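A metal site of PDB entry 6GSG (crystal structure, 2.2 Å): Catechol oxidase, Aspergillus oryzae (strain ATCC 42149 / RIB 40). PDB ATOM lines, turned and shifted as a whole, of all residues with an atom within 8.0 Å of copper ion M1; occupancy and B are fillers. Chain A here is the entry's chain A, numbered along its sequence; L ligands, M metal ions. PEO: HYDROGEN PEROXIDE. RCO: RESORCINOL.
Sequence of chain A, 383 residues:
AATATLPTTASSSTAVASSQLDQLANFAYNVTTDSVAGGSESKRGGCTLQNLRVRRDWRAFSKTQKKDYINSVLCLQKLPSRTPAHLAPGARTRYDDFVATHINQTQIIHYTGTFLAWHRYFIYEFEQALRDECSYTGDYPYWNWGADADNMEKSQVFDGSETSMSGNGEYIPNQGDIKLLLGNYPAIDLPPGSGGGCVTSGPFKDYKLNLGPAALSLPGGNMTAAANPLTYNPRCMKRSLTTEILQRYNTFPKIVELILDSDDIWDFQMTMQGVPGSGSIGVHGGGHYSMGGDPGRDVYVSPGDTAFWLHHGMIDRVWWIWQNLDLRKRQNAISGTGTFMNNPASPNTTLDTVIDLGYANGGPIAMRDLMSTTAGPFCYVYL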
ATOM      1  N   HIS A 102      -2.660  17.991 -29.363  1.00  0.00           N
ATOM      2  CA  HIS A 102      -4.103  17.783 -29.222  1.00  0.00           C
ATOM      3  C   HIS A 102      -4.759  17.573 -30.581  1.00  0.00           C
ATOM      4  O   HIS A 102      -5.615  16.698 -30.741  1.00  0.00           O
ATOM      5  CB  HIS A 102      -4.729  18.977 -28.491  1.00  0.00           C
ATOM      6  CG  HIS A 102      -6.160  18.765 -28.110  1.00  0.00           C
ATOM      7  ND1 HIS A 102      -7.195  18.955 -29.004  1.00  0.00           N
ATOM      8  CD2 HIS A 102      -6.729  18.353 -26.962  1.00  0.00           C
ATOM      9  CE1 HIS A 102      -8.342  18.699 -28.401  1.00  0.00           C
ATOM     10  NE2 HIS A 102      -8.089  18.314 -27.168  1.00  0.00           N
ATOM     11  N   ILE A 109      -8.500  10.611 -28.026  1.00  0.00           N
ATOM     12  CA  ILE A 109      -8.572  11.192 -26.682  1.00  0.00           C
ATOM     13  C   ILE A 109      -9.940  11.752 -26.356  1.00  0.00           C
ATOM     14  O   ILE A 109     -10.119  12.334 -25.278  1.00  0.00           O
ATOM     15  CB  ILE A 109      -7.489  12.275 -26.474  1.00  0.00           C
ATOM     16  CG1 ILE A 109      -7.687  13.424 -27.460  1.00  0.00           C
ATOM     17  CG2 ILE A 109      -6.095  11.683 -26.589  1.00  0.00           C
ATOM     18  CD1 ILE A 109      -6.708  14.555 -27.293  1.00  0.00           C
ATOM     19  N   HIS A 110     -10.930  11.611 -27.246  1.00  0.00           N
ATOM     20  CA  HIS A 110     -12.291  12.023 -26.980  1.00  0.00           C
ATOM     21  C   HIS A 110     -13.219  10.841 -27.222  1.00  0.00           C
ATOM     22  O   HIS A 110     -13.030  10.082 -28.179  1.00  0.00           O
ATOM     23  CB  HIS A 110     -12.695  13.222 -27.866  1.00  0.00           C
ATOM     24  CG  HIS A 110     -11.852  14.437 -27.643  1.00  0.00           C
ATOM     25  ND1 HIS A 110     -10.811  14.790 -28.494  1.00  0.00           N
ATOM     26  CD2 HIS A 110     -11.866  15.379 -26.663  1.00  0.00           C
ATOM     27  CE1 HIS A 110     -10.243  15.902 -28.051  1.00  0.00           C
ATOM     28  NE2 HIS A 110     -10.861  16.272 -26.938  1.00  0.00           N
ATOM     29  N   PHE A 115     -10.243   9.551 -22.127  1.00  0.00           N
ATOM     30  CA  PHE A 115     -10.608  10.960 -22.240  1.00  0.00           C
ATOM     31  C   PHE A 115     -10.265  11.744 -20.966  1.00  0.00           C
ATOM     32  O   PHE A 115      -9.547  12.750 -21.015  1.00  0.00           O
ATOM     33  CB  PHE A 115     -12.090  11.098 -22.575  1.00  0.00           C
ATOM     34  CG  PHE A 115     -12.651  12.471 -22.345  1.00  0.00           C
ATOM     35  CD1 PHE A 115     -12.263  13.535 -23.148  1.00  0.00           C
ATOM     36  CD2 PHE A 115     -13.563  12.715 -21.323  1.00  0.00           C
ATOM     37  CE1 PHE A 115     -12.776  14.817 -22.944  1.00  0.00           C
ATOM     38  CE2 PHE A 115     -14.082  13.987 -21.113  1.00  0.00           C
ATOM     39  CZ  PHE A 115     -13.682  15.037 -21.925  1.00  0.00           C
ATOM     40  N   HIS A 119      -6.735  14.149 -20.361  1.00  0.00           N
ATOM     41  CA  HIS A 119      -6.865  15.595 -20.172  1.00  0.00           C
ATOM     42  C   HIS A 119      -6.360  16.023 -18.808  1.00  0.00           C
ATOM     43  O   HIS A 119      -5.868  17.150 -18.653  1.00  0.00           O
ATOM     44  CB  HIS A 119      -8.314  16.020 -20.403  1.00  0.00           C
ATOM     45  CG  HIS A 119      -8.683  16.087 -21.855  1.00  0.00           C
ATOM     46  ND1 HIS A 119      -9.062  14.972 -22.578  1.00  0.00           N
ATOM     47  CD2 HIS A 119      -8.696  17.115 -22.731  1.00  0.00           C
ATOM     48  CE1 HIS A 119      -9.313  15.326 -23.829  1.00  0.00           C
ATOM     49  NE2 HIS A 119      -9.099  16.618 -23.948  1.00  0.00           N
ATOM     50  N   GLN A 273     -19.637  14.528 -21.712  1.00  0.00           N
ATOM     51  CA  GLN A 273     -19.341  14.919 -23.086  1.00  0.00           C
ATOM     52  C   GLN A 273     -20.594  15.070 -23.937  1.00  0.00           C
ATOM     53  O   GLN A 273     -20.546  15.720 -24.991  1.00  0.00           O
ATOM     54  CB  GLN A 273     -18.408  13.902 -23.734  1.00  0.00           C
ATOM     55  CG  GLN A 273     -17.126  13.660 -22.952  1.00  0.00           C
ATOM     56  CD  GLN A 273     -16.335  12.485 -23.478  1.00  0.00           C
ATOM     57  OE1 GLN A 273     -15.601  12.603 -24.455  1.00  0.00           O
ATOM     58  NE2 GLN A 273     -16.482  11.336 -22.829  1.00  0.00           N
ATOM     59  N   VAL A 283     -21.752  19.264 -20.015  1.00  0.00           N
ATOM     60  CA  VAL A 283     -20.988  20.400 -19.501  1.00  0.00           C
ATOM     61  C   VAL A 283     -19.719  20.593 -20.321  1.00  0.00           C
ATOM     62  O   VAL A 283     -19.254  21.731 -20.493  1.00  0.00           O
ATOM     63  CB  VAL A 283     -20.677  20.230 -18.000  1.00  0.00           C
ATOM     64  CG1 VAL A 283     -21.952  20.213 -17.174  1.00  0.00           C
ATOM     65  CG2 VAL A 283     -19.842  18.970 -17.743  1.00  0.00           C
ATOM     66  N   HIS A 284     -19.144  19.507 -20.851  1.00  0.00           N
ATOM     67  CA  HIS A 284     -17.912  19.622 -21.634  1.00  0.00           C
ATOM     68  C   HIS A 284     -18.158  20.383 -22.930  1.00  0.00           C
ATOM     69  O   HIS A 284     -17.549  21.429 -23.176  1.00  0.00           O
ATOM     70  CB  HIS A 284     -17.345  18.236 -21.920  1.00  0.00           C
ATOM     71  CG  HIS A 284     -16.082  18.263 -22.713  1.00  0.00           C
ATOM     72  ND1 HIS A 284     -15.987  17.698 -23.972  1.00  0.00           N
ATOM     73  CD2 HIS A 284     -14.867  18.783 -22.440  1.00  0.00           C
ATOM     74  CE1 HIS A 284     -14.762  17.867 -24.432  1.00  0.00           C
ATOM     75  NE2 HIS A 284     -14.061  18.525 -23.525  1.00  0.00           N
ATOM     76  N   GLY A 285     -19.057  19.874 -23.776  1.00  0.00           N
ATOM     77  CA  GLY A 285     -19.365  20.573 -25.021  1.00  0.00           C
ATOM     78  C   GLY A 285     -19.978  21.929 -24.788  1.00  0.00           C
ATOM     79  O   GLY A 285     -19.709  22.886 -25.527  1.00  0.00           O
ATOM     80  N   GLY A 287     -19.435  24.066 -22.264  1.00  0.00           N
ATOM     81  CA  GLY A 287     -18.391  25.019 -21.931  1.00  0.00           C
ATOM     82  C   GLY A 287     -17.544  25.410 -23.135  1.00  0.00           C
ATOM     83  O   GLY A 287     -17.146  26.564 -23.282  1.00  0.00           O
ATOM     84  N   HIS A 288     -17.262  24.440 -24.009  1.00  0.00           N
ATOM     85  CA  HIS A 288     -16.464  24.709 -25.210  1.00  0.00           C
ATOM     86  C   HIS A 288     -17.211  25.641 -26.161  1.00  0.00           C
ATOM     87  O   HIS A 288     -16.733  26.729 -26.492  1.00  0.00           O
ATOM     88  CB  HIS A 288     -16.129  23.393 -25.915  1.00  0.00           C
ATOM     89  CG  HIS A 288     -14.859  22.750 -25.445  1.00  0.00           C
ATOM     90  ND1 HIS A 288     -13.628  23.368 -25.541  1.00  0.00           N
ATOM     91  CD2 HIS A 288     -14.623  21.545 -24.884  1.00  0.00           C
ATOM     92  CE1 HIS A 288     -12.700  22.571 -25.062  1.00  0.00           C
ATOM     93  NE2 HIS A 288     -13.275  21.459 -24.650  1.00  0.00           N
ATOM     94  N   MET A 291     -17.938  29.571 -25.889  1.00  0.00           N
ATOM     95  CA  MET A 291     -16.936  30.561 -26.273  1.00  0.00           C
ATOM     96  C   MET A 291     -17.131  31.034 -27.717  1.00  0.00           C
ATOM     97  O   MET A 291     -16.730  32.159 -28.044  1.00  0.00           O
ATOM     98  CB  MET A 291     -15.529  29.975 -26.121  1.00  0.00           C
ATOM     99  CG  MET A 291     -15.268  29.257 -24.805  1.00  0.00           C
ATOM    100  SD  MET A 291     -13.604  28.555 -24.767  1.00  0.00           S
ATOM    101  CE  MET A 291     -13.739  27.407 -23.384  1.00  0.00           C
ATOM    102  N   VAL A 299     -12.966  21.105 -32.492  1.00  0.00           N
ATOM    103  CA  VAL A 299     -12.631  20.076 -31.507  1.00  0.00           C
ATOM    104  C   VAL A 299     -11.125  19.814 -31.503  1.00  0.00           C
ATOM    105  O   VAL A 299     -10.531  19.567 -30.440  1.00  0.00           O
ATOM    106  CB  VAL A 299     -13.443  18.801 -31.794  1.00  0.00           C
ATOM    107  CG1 VAL A 299     -13.004  17.664 -30.870  1.00  0.00           C
ATOM    108  CG2 VAL A 299     -14.922  19.060 -31.643  1.00  0.00           C
ATOM    109  N   SER A 302      -9.091  23.248 -30.106  1.00  0.00           N
ATOM    110  CA  SER A 302      -9.652  23.958 -28.970  1.00  0.00           C
ATOM    111  C   SER A 302      -8.635  24.470 -27.951  1.00  0.00           C
ATOM    112  O   SER A 302      -8.852  25.562 -27.400  1.00  0.00           O
ATOM    113  CB  SER A 302     -10.694  23.080 -28.257  1.00  0.00           C
ATOM    114  OG  SER A 302     -10.157  21.820 -27.881  1.00  0.00           O
ATOM    115  N   PRO A 303      -7.517  23.783 -27.656  1.00  0.00           N
ATOM    116  CA  PRO A 303      -6.520  24.402 -26.761  1.00  0.00           C
ATOM    117  C   PRO A 303      -5.971  25.737 -27.253  1.00  0.00           C
ATOM    118  O   PRO A 303      -5.371  26.473 -26.465  1.00  0.00           O
ATOM    119  CB  PRO A 303      -5.406  23.345 -26.669  1.00  0.00           C
ATOM    120  CG  PRO A 303      -6.109  22.071 -26.935  1.00  0.00           C
ATOM    121  CD  PRO A 303      -7.120  22.399 -27.981  1.00  0.00           C
ATOM    122  N   PHE A 308      -9.393  27.344 -22.590  1.00  0.00           N
ATOM    123  CA  PHE A 308      -9.379  25.882 -22.550  1.00  0.00           C
ATOM    124  C   PHE A 308      -8.836  25.356 -21.220  1.00  0.00           C
ATOM    125  O   PHE A 308      -9.377  24.398 -20.650  1.00  0.00           O
ATOM    126  CB  PHE A 308      -8.548  25.340 -23.717  1.00  0.00           C
ATOM    127  CG  PHE A 308      -8.329  23.845 -23.698  1.00  0.00           C
ATOM    128  CD1 PHE A 308      -7.302  23.293 -22.944  1.00  0.00           C
ATOM    129  CD2 PHE A 308      -9.124  23.009 -24.459  1.00  0.00           C
ATOM    130  CE1 PHE A 308      -7.101  21.925 -22.932  1.00  0.00           C
ATOM    131  CE2 PHE A 308      -8.925  21.645 -24.456  1.00  0.00           C
ATOM    132  CZ  PHE A 308      -7.908  21.101 -23.683  1.00  0.00           C
ATOM    133  N   HIS A 311     -11.282  25.826 -18.405  1.00  0.00           N
ATOM    134  CA  HIS A 311     -12.439  24.981 -18.627  1.00  0.00           C
ATOM    135  C   HIS A 311     -12.151  23.540 -18.221  1.00  0.00           C
ATOM    136  O   HIS A 311     -12.971  22.886 -17.566  1.00  0.00           O
ATOM    137  CB  HIS A 311     -12.868  25.064 -20.090  1.00  0.00           C
ATOM    138  CG  HIS A 311     -13.892  24.048 -20.498  1.00  0.00           C
ATOM    139  ND1 HIS A 311     -15.105  23.925 -19.863  1.00  0.00           N
ATOM    140  CD2 HIS A 311     -13.889  23.128 -21.498  1.00  0.00           C
ATOM    141  CE1 HIS A 311     -15.807  22.959 -20.450  1.00  0.00           C
ATOM    142  NE2 HIS A 311     -15.088  22.459 -21.438  1.00  0.00           N
ATOM    143  N   HIS A 312     -10.971  23.036 -18.575  1.00  0.00           N
ATOM    144  CA  HIS A 312     -10.636  21.655 -18.253  1.00  0.00           C
ATOM    145  C   HIS A 312     -10.121  21.483 -16.837  1.00  0.00           C
ATOM    146  O   HIS A 312     -10.141  20.363 -16.319  1.00  0.00           O
ATOM    147  CB  HIS A 312      -9.626  21.108 -19.268  1.00  0.00           C
ATOM    148  CG  HIS A 312     -10.277  20.423 -20.423  1.00  0.00           C
ATOM    149  ND1 HIS A 312     -10.693  19.112 -20.371  1.00  0.00           N
ATOM    150  CD2 HIS A 312     -10.641  20.886 -21.645  1.00  0.00           C
ATOM    151  CE1 HIS A 312     -11.246  18.783 -21.517  1.00  0.00           C
ATOM    152  NE2 HIS A 312     -11.234  19.841 -22.302  1.00  0.00           N
ATOM    153  N   ILE A 315     -13.445  20.691 -15.524  1.00  0.00           N
ATOM    154  CA  ILE A 315     -13.760  19.311 -15.908  1.00  0.00           C
ATOM    155  C   ILE A 315     -13.066  18.333 -14.958  1.00  0.00           C
ATOM    156  O   ILE A 315     -13.685  17.378 -14.461  1.00  0.00           O
ATOM    157  CB  ILE A 315     -13.345  19.056 -17.364  1.00  0.00           C
ATOM    158  CG1 ILE A 315     -14.252  19.818 -18.335  1.00  0.00           C
ATOM    159  CG2 ILE A 315     -13.346  17.560 -17.678  1.00  0.00           C
ATOM    160  CD1 ILE A 315     -15.613  19.178 -18.559  1.00  0.00           C
HETATM  161  O1  PEO L   1     -11.483  19.437 -26.811  1.00  0.00           O
HETATM  162  O2  PEO L   1     -11.208  18.856 -25.517  1.00  0.00           O
HETATM  163  C1  RCO L   2     -14.509  19.307 -27.704  1.00  0.00           C
HETATM  164  C2  RCO L   2     -13.957  20.505 -28.133  1.00  0.00           C
HETATM  165  C3  RCO L   2     -14.780  21.515 -28.612  1.00  0.00           C
HETATM  166  C4  RCO L   2     -16.153  21.326 -28.677  1.00  0.00           C
HETATM  167  C5  RCO L   2     -16.697  20.118 -28.244  1.00  0.00           C
HETATM  168  C6  RCO L   2     -15.887  19.108 -27.761  1.00  0.00           C
HETATM  169  O1  RCO L   2     -13.700  18.319 -27.232  1.00  0.00           O
HETATM  170  O3  RCO L   2     -14.228  22.695 -29.039  1.00  0.00           O
HETATM  171 CU    CU M   1     -12.455  19.764 -23.883  1.00  0.00          CU
HETATM  172 CU    CU M   2      -9.296  17.479 -25.819  1.00  0.00          CU
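The backbone carbonyl oxygen (O) of His 284 sits at hydrogen-bond distance from a ring nitrogen (NE2) of His 311 (3.2 Å).
Of the 19 residues printed, 3 come within 4 Å of copper ion M1.
Copper ion M1 is bound by a ring nitrogen (NE2) of His 312 (2.0 Å), a ring nitrogen (NE2) of His 288 (2.0 Å), a ring nitrogen (NE2) of His 284 (2.1 Å) and an oxygen (O2) of PEO L1 (2.2 Å).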
